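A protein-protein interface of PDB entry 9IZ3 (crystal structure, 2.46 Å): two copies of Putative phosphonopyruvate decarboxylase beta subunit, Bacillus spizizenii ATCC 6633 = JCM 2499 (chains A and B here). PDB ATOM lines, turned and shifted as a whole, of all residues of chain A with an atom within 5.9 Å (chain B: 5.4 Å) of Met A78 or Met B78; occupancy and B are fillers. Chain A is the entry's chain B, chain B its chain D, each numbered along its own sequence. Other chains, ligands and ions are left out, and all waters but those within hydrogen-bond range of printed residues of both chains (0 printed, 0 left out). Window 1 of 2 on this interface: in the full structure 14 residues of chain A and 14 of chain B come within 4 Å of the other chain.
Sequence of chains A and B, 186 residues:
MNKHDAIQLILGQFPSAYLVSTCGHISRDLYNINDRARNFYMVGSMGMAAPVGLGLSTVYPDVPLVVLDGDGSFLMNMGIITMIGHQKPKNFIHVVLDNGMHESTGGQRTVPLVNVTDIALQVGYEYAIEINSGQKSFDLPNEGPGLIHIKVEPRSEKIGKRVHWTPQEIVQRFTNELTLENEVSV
Ser A73 touches none of the printed residues of chain B. Met A76 touches none of the printed residues of chain B. Of chain B, only Met B78, Gly B79 and Thr B82 come within 4 Å of Met A78. Of the printed residues of chain B, Val A123 touches Ile B119. Of the printed residues of chain A, Met B78 touches Met A78 (3.6 Å), Gly A79 (3.7 Å) and Thr A82 (3.8 Å). Of the printed residues of chain A, Gly B79 touches Met A78. Of the printed residues of chain A, Thr B82 touches Met A78. Of the printed residues of chain A, Ile B119 touches Val A123. Of the printed residues of chain A, Val B123 touches Ile A119. The nearest residue of chain A that does not touch Met B78 is Ile A81 (4.1 Å). The nearest printed residue of chain A that does not touch Gly B79 is Leu A75 (4.7 Å).
Met A78 touches Gly B79, and with the chains exchanged Gly A79 touches Met B78. Met A78 touches Thr B82, and with the chains exchanged Thr A82 touches Met B78. Thr A82 touches Leu B75, but with the chains exchanged Leu A75 does not touch Thr B82 (4.02 Å). Ile A119 touches Val B123, and with the chains exchanged Val A123 touches Ile B119. Positions printed for both chains: 74, 75, 76, 77, 78, 79, 80, 81, 82, 119 and 123.
Met A78 touches Met B78. CE of Met A78 touches CA of Gly B79, at 3.8 Å. SD of Met A78 touches CG2 of Thr B82, at 3.7 Å. Gly A79 touches Met B78. CG2 of Thr A82 touches CD2 of Leu B75, at 3.7 Å. CG2 of Thr A82 touches SD of Met B78 (3.8 Å). Val B123 touches Ile A119 (CG1 to CD1, 3.7 Å). CG1 of Val A123 touches CD1 of Ile B119, 3.7 Å away.
Printed residues of chain B that touch a printed residue of chain A: Leu B75, Met B78, Gly B79, Thr B82, Ile B119 and Val B123. Hydrophobic or aromatic side chains of chain B that line the printed part of chain A: Leu B75, Met B78, Ile B119 and Val B123. Printed residues of chain A that touch a printed residue of chain B: Met A78, Gly A79, Thr A82, Ile A119 and Val A123. Among the printed residues, 8 pairs touch across the chains. Among the printed residues, no Asp or Glu carboxylate lies within 4 Å of a Lys or Arg side-chain nitrogen of the other chain.
The side-chain hydroxyl (OG1) of Thr B82 lies within hydrogen-bond range of the backbone carbonyl oxygen (O) of Gly B79 (2.5 Å).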
ATOM      1  N   SER A  73      -9.287 -13.422 -24.811  1.00  0.00           N
ATOM      2  CA  SER A  73     -10.138 -12.848 -23.777  1.00  0.00           C
ATOM      3  C   SER A  73     -11.208 -11.952 -24.380  1.00  0.00           C
ATOM      4  O   SER A  73     -12.332 -11.899 -23.871  1.00  0.00           O
ATOM      5  CB  SER A  73      -9.293 -12.074 -22.763  1.00  0.00           C
ATOM      6  OG  SER A  73      -8.885 -10.819 -23.285  1.00  0.00           O
ATOM      7  N   PHE A  74     -10.884 -11.249 -25.469  1.00  0.00           N
ATOM      8  CA  PHE A  74     -11.895 -10.452 -26.154  1.00  0.00           C
ATOM      9  C   PHE A  74     -13.017 -11.333 -26.700  1.00  0.00           C
ATOM     10  O   PHE A  74     -14.201 -11.047 -26.488  1.00  0.00           O
ATOM     11  CB  PHE A  74     -11.260  -9.640 -27.280  1.00  0.00           C
ATOM     12  CG  PHE A  74     -12.216  -8.702 -27.954  1.00  0.00           C
ATOM     13  CD1 PHE A  74     -12.965  -9.114 -29.041  1.00  0.00           C
ATOM     14  CD2 PHE A  74     -12.379  -7.407 -27.485  1.00  0.00           C
ATOM     15  CE1 PHE A  74     -13.853  -8.253 -29.654  1.00  0.00           C
ATOM     16  CE2 PHE A  74     -13.265  -6.543 -28.093  1.00  0.00           C
ATOM     17  CZ  PHE A  74     -14.004  -6.965 -29.176  1.00  0.00           C
ATOM     18  N   LEU A  75     -12.664 -12.408 -27.414  1.00  0.00           N
ATOM     19  CA  LEU A  75     -13.696 -13.229 -28.047  1.00  0.00           C
ATOM     20  C   LEU A  75     -14.511 -14.004 -27.020  1.00  0.00           C
ATOM     21  O   LEU A  75     -15.702 -14.254 -27.239  1.00  0.00           O
ATOM     22  CB  LEU A  75     -13.064 -14.191 -29.054  1.00  0.00           C
ATOM     23  CG  LEU A  75     -12.641 -13.611 -30.408  1.00  0.00           C
ATOM     24  CD1 LEU A  75     -11.882 -14.655 -31.211  1.00  0.00           C
ATOM     25  CD2 LEU A  75     -13.845 -13.102 -31.199  1.00  0.00           C
ATOM     26  N   MET A  76     -13.897 -14.370 -25.893  1.00  0.00           N
ATOM     27  CA  MET A  76     -14.586 -15.189 -24.901  1.00  0.00           C
ATOM     28  C   MET A  76     -15.795 -14.471 -24.315  1.00  0.00           C
ATOM     29  O   MET A  76     -16.822 -15.100 -24.033  1.00  0.00           O
ATOM     30  CB  MET A  76     -13.611 -15.587 -23.797  1.00  0.00           C
ATOM     31  CG  MET A  76     -14.248 -16.365 -22.664  1.00  0.00           C
ATOM     32  SD  MET A  76     -13.012 -17.117 -21.597  1.00  0.00           S
ATOM     33  CE  MET A  76     -12.097 -18.081 -22.796  1.00  0.00           C
ATOM     34  N   ASN A  77     -15.693 -13.158 -24.113  1.00  0.00           N
ATOM     35  CA  ASN A  77     -16.784 -12.365 -23.555  1.00  0.00           C
ATOM     36  C   ASN A  77     -17.044 -11.161 -24.460  1.00  0.00           C
ATOM     37  O   ASN A  77     -16.944 -10.012 -24.045  1.00  0.00           O
ATOM     38  CB  ASN A  77     -16.460 -11.931 -22.120  1.00  0.00           C
ATOM     39  CG  ASN A  77     -17.639 -11.271 -21.420  1.00  0.00           C
ATOM     40  OD1 ASN A  77     -18.798 -11.497 -21.777  1.00  0.00           O
ATOM     41  ND2 ASN A  77     -17.346 -10.455 -20.411  1.00  0.00           N
ATOM     42  N   MET A  78     -17.387 -11.431 -25.722  1.00  0.00           N
ATOM     43  CA  MET A  78     -17.525 -10.341 -26.687  1.00  0.00           C
ATOM     44  C   MET A  78     -18.698  -9.429 -26.350  1.00  0.00           C
ATOM     45  O   MET A  78     -18.619  -8.212 -26.568  1.00  0.00           O
ATOM     46  CB  MET A  78     -17.674 -10.901 -28.102  1.00  0.00           C
ATOM     47  CG  MET A  78     -17.287  -9.908 -29.188  1.00  0.00           C
ATOM     48  SD  MET A  78     -17.539 -10.528 -30.863  1.00  0.00           S
ATOM     49  CE  MET A  78     -19.282 -10.915 -30.823  1.00  0.00           C
ATOM     50  N   GLY A  79     -19.772  -9.989 -25.798  1.00  0.00           N
ATOM     51  CA  GLY A  79     -20.962  -9.231 -25.459  1.00  0.00           C
ATOM     52  C   GLY A  79     -20.718  -7.993 -24.620  1.00  0.00           C
ATOM     53  O   GLY A  79     -21.513  -7.047 -24.667  1.00  0.00           O
ATOM     54  N   ILE A  80     -19.613  -7.979 -23.864  1.00  0.00           N
ATOM     55  CA  ILE A  80     -19.284  -6.822 -23.033  1.00  0.00           C
ATOM     56  C   ILE A  80     -19.299  -5.542 -23.853  1.00  0.00           C
ATOM     57  O   ILE A  80     -19.717  -4.484 -23.360  1.00  0.00           O
ATOM     58  CB  ILE A  80     -17.922  -7.022 -22.327  1.00  0.00           C
ATOM     59  CG1 ILE A  80     -17.634  -5.856 -21.391  1.00  0.00           C
ATOM     60  CG2 ILE A  80     -16.790  -7.076 -23.336  1.00  0.00           C
ATOM     61  CD1 ILE A  80     -18.341  -5.940 -20.091  1.00  0.00           C
ATOM     62  N   ILE A  81     -18.887  -5.614 -25.122  1.00  0.00           N
ATOM     63  CA  ILE A  81     -18.790  -4.394 -25.919  1.00  0.00           C
ATOM     64  C   ILE A  81     -20.150  -3.713 -26.021  1.00  0.00           C
ATOM     65  O   ILE A  81     -20.244  -2.480 -25.983  1.00  0.00           O
ATOM     66  CB  ILE A  81     -18.182  -4.694 -27.305  1.00  0.00           C
ATOM     67  CG1 ILE A  81     -19.117  -5.555 -28.155  1.00  0.00           C
ATOM     68  CG2 ILE A  81     -16.832  -5.371 -27.152  1.00  0.00           C
ATOM     69  CD1 ILE A  81     -18.600  -5.787 -29.553  1.00  0.00           C
ATOM     70  N   THR A  82     -21.229  -4.502 -26.080  1.00  0.00           N
ATOM     71  CA  THR A  82     -22.562  -3.914 -26.168  1.00  0.00           C
ATOM     72  C   THR A  82     -22.831  -2.993 -24.988  1.00  0.00           C
ATOM     73  O   THR A  82     -23.402  -1.909 -25.150  1.00  0.00           O
ATOM     74  CB  THR A  82     -23.621  -5.010 -26.225  1.00  0.00           C
ATOM     75  OG1 THR A  82     -23.437  -5.895 -25.112  1.00  0.00           O
ATOM     76  CG2 THR A  82     -23.510  -5.787 -27.535  1.00  0.00           C
ATOM     77  N   ILE A 119     -16.858  -3.500 -35.762  1.00  0.00           N
ATOM     78  CA  ILE A 119     -17.886  -3.962 -34.830  1.00  0.00           C
ATOM     79  C   ILE A 119     -17.930  -3.074 -33.592  1.00  0.00           C
ATOM     80  O   ILE A 119     -19.012  -2.760 -33.069  1.00  0.00           O
ATOM     81  CB  ILE A 119     -17.634  -5.440 -34.469  1.00  0.00           C
ATOM     82  CG1 ILE A 119     -17.820  -6.335 -35.691  1.00  0.00           C
ATOM     83  CG2 ILE A 119     -18.545  -5.909 -33.337  1.00  0.00           C
ATOM     84  CD1 ILE A 119     -17.251  -7.726 -35.503  1.00  0.00           C
ATOM     85  N   VAL A 123     -21.341  -1.077 -32.302  1.00  0.00           N
ATOM     86  CA  VAL A 123     -22.029  -1.137 -31.010  1.00  0.00           C
ATOM     87  C   VAL A 123     -21.964   0.165 -30.228  1.00  0.00           C
ATOM     88  O   VAL A 123     -22.474   0.221 -29.101  1.00  0.00           O
ATOM     89  CB  VAL A 123     -21.466  -2.262 -30.124  1.00  0.00           C
ATOM     90  CG1 VAL A 123     -21.580  -3.600 -30.844  1.00  0.00           C
ATOM     91  CG2 VAL A 123     -20.025  -1.955 -29.744  1.00  0.00           C
ATOM     92  N   PHE B  74     -29.936 -13.521 -27.533  1.00  0.00           N
ATOM     93  CA  PHE B  74     -28.862 -13.226 -28.473  1.00  0.00           C
ATOM     94  C   PHE B  74     -27.713 -12.504 -27.776  1.00  0.00           C
ATOM     95  O   PHE B  74     -26.546 -12.886 -27.919  1.00  0.00           O
ATOM     96  CB  PHE B  74     -29.401 -12.395 -29.637  1.00  0.00           C
ATOM     97  CG  PHE B  74     -28.387 -12.115 -30.708  1.00  0.00           C
ATOM     98  CD1 PHE B  74     -28.125 -13.052 -31.694  1.00  0.00           C
ATOM     99  CD2 PHE B  74     -27.700 -10.913 -30.731  1.00  0.00           C
ATOM    100  CE1 PHE B  74     -27.195 -12.800 -32.682  1.00  0.00           C
ATOM    101  CE2 PHE B  74     -26.768 -10.653 -31.717  1.00  0.00           C
ATOM    102  CZ  PHE B  74     -26.514 -11.599 -32.694  1.00  0.00           C
ATOM    103  N   LEU B  75     -28.030 -11.457 -27.010  1.00  0.00           N
ATOM    104  CA  LEU B  75     -26.989 -10.710 -26.312  1.00  0.00           C
ATOM    105  C   LEU B  75     -26.286 -11.564 -25.267  1.00  0.00           C
ATOM    106  O   LEU B  75     -25.081 -11.406 -25.044  1.00  0.00           O
ATOM    107  CB  LEU B  75     -27.592  -9.466 -25.661  1.00  0.00           C
ATOM    108  CG  LEU B  75     -27.918  -8.288 -26.580  1.00  0.00           C
ATOM    109  CD1 LEU B  75     -28.754  -7.265 -25.837  1.00  0.00           C
ATOM    110  CD2 LEU B  75     -26.646  -7.648 -27.102  1.00  0.00           C
ATOM    111  N   MET B  76     -27.016 -12.482 -24.629  1.00  0.00           N
ATOM    112  CA  MET B  76     -26.441 -13.284 -23.557  1.00  0.00           C
ATOM    113  C   MET B  76     -25.277 -14.137 -24.042  1.00  0.00           C
ATOM    114  O   MET B  76     -24.367 -14.445 -23.264  1.00  0.00           O
ATOM    115  CB  MET B  76     -27.522 -14.166 -22.931  1.00  0.00           C
ATOM    116  CG  MET B  76     -27.081 -14.874 -21.663  1.00  0.00           C
ATOM    117  SD  MET B  76     -28.434 -15.216 -20.528  1.00  0.00           S
ATOM    118  CE  MET B  76     -29.251 -13.625 -20.486  1.00  0.00           C
ATOM    119  N   ASN B  77     -25.283 -14.532 -25.321  1.00  0.00           N
ATOM    120  CA  ASN B  77     -24.219 -15.344 -25.900  1.00  0.00           C
ATOM    121  C   ASN B  77     -23.959 -14.824 -27.320  1.00  0.00           C
ATOM    122  O   ASN B  77     -24.174 -15.508 -28.313  1.00  0.00           O
ATOM    123  CB  ASN B  77     -24.587 -16.829 -25.892  1.00  0.00           C
ATOM    124  CG  ASN B  77     -23.423 -17.729 -26.270  1.00  0.00           C
ATOM    125  OD1 ASN B  77     -22.257 -17.375 -26.083  1.00  0.00           O
ATOM    126  ND2 ASN B  77     -23.737 -18.907 -26.806  1.00  0.00           N
ATOM    127  N   MET B  78     -23.485 -13.578 -27.415  1.00  0.00           N
ATOM    128  CA  MET B  78     -23.310 -12.955 -28.723  1.00  0.00           C
ATOM    129  C   MET B  78     -22.130 -13.554 -29.479  1.00  0.00           C
ATOM    130  O   MET B  78     -22.197 -13.730 -30.702  1.00  0.00           O
ATOM    131  CB  MET B  78     -23.129 -11.444 -28.572  1.00  0.00           C
ATOM    132  CG  MET B  78     -23.275 -10.692 -29.884  1.00  0.00           C
ATOM    133  SD  MET B  78     -23.138  -8.900 -29.723  1.00  0.00           S
ATOM    134  CE  MET B  78     -21.490  -8.750 -29.051  1.00  0.00           C
ATOM    135  N   GLY B  79     -21.051 -13.892 -28.769  1.00  0.00           N
ATOM    136  CA  GLY B  79     -19.847 -14.387 -29.416  1.00  0.00           C
ATOM    137  C   GLY B  79     -20.048 -15.621 -30.277  1.00  0.00           C
ATOM    138  O   GLY B  79     -19.192 -15.922 -31.118  1.00  0.00           O
ATOM    139  N   ILE B  80     -21.161 -16.340 -30.095  1.00  0.00           N
ATOM    140  CA  ILE B  80     -21.443 -17.501 -30.937  1.00  0.00           C
ATOM    141  C   ILE B  80     -21.481 -17.105 -32.408  1.00  0.00           C
ATOM    142  O   ILE B  80     -21.155 -17.920 -33.284  1.00  0.00           O
ATOM    143  CB  ILE B  80     -22.758 -18.182 -30.505  1.00  0.00           C
ATOM    144  CG1 ILE B  80     -22.928 -19.532 -31.210  1.00  0.00           C
ATOM    145  CG2 ILE B  80     -23.954 -17.292 -30.814  1.00  0.00           C
ATOM    146  CD1 ILE B  80     -21.812 -20.513 -30.938  1.00  0.00           C
ATOM    147  N   ILE B  81     -21.851 -15.855 -32.708  1.00  0.00           N
ATOM    148  CA  ILE B  81     -21.904 -15.430 -34.102  1.00  0.00           C
ATOM    149  C   ILE B  81     -20.525 -15.531 -34.740  1.00  0.00           C
ATOM    150  O   ILE B  81     -20.397 -15.890 -35.916  1.00  0.00           O
ATOM    151  CB  ILE B  81     -22.487 -14.008 -34.223  1.00  0.00           C
ATOM    152  CG1 ILE B  81     -21.549 -12.975 -33.587  1.00  0.00           C
ATOM    153  CG2 ILE B  81     -23.888 -13.951 -33.610  1.00  0.00           C
ATOM    154  CD1 ILE B  81     -21.968 -11.551 -33.817  1.00  0.00           C
ATOM    155  N   THR B  82     -19.467 -15.261 -33.966  1.00  0.00           N
ATOM    156  CA  THR B  82     -18.124 -15.365 -34.525  1.00  0.00           C
ATOM    157  C   THR B  82     -17.819 -16.790 -34.940  1.00  0.00           C
ATOM    158  O   THR B  82     -17.030 -17.012 -35.866  1.00  0.00           O
ATOM    159  CB  THR B  82     -17.078 -14.899 -33.520  1.00  0.00           C
ATOM    160  OG1 THR B  82     -17.028 -15.836 -32.434  1.00  0.00           O
ATOM    161  CG2 THR B  82     -17.415 -13.505 -33.007  1.00  0.00           C
ATOM    162  N   ILE B 119     -23.300  -6.246 -37.759  1.00  0.00           N
ATOM    163  CA  ILE B 119     -22.334  -7.016 -36.981  1.00  0.00           C
ATOM    164  C   ILE B 119     -22.276  -8.457 -37.476  1.00  0.00           C
ATOM    165  O   ILE B 119     -21.188  -9.036 -37.631  1.00  0.00           O
ATOM    166  CB  ILE B 119     -22.684  -6.929 -35.483  1.00  0.00           C
ATOM    167  CG1 ILE B 119     -22.538  -5.487 -34.991  1.00  0.00           C
ATOM    168  CG2 ILE B 119     -21.801  -7.857 -34.659  1.00  0.00           C
ATOM    169  CD1 ILE B 119     -23.246  -5.208 -33.677  1.00  0.00           C
ATOM    170  N   VAL B 123     -18.908 -10.404 -38.978  1.00  0.00           N
ATOM    171  CA  VAL B 123     -18.292 -11.637 -38.482  1.00  0.00           C
ATOM    172  C   VAL B 123     -18.340 -12.785 -39.486  1.00  0.00           C
ATOM    173  O   VAL B 123     -17.760 -13.848 -39.218  1.00  0.00           O
ATOM    174  CB  VAL B 123     -18.929 -12.122 -37.163  1.00  0.00           C
ATOM    175  CG1 VAL B 123     -18.837 -11.032 -36.090  1.00  0.00           C
ATOM    176  CG2 VAL B 123     -20.370 -12.564 -37.385  1.00  0.00           C
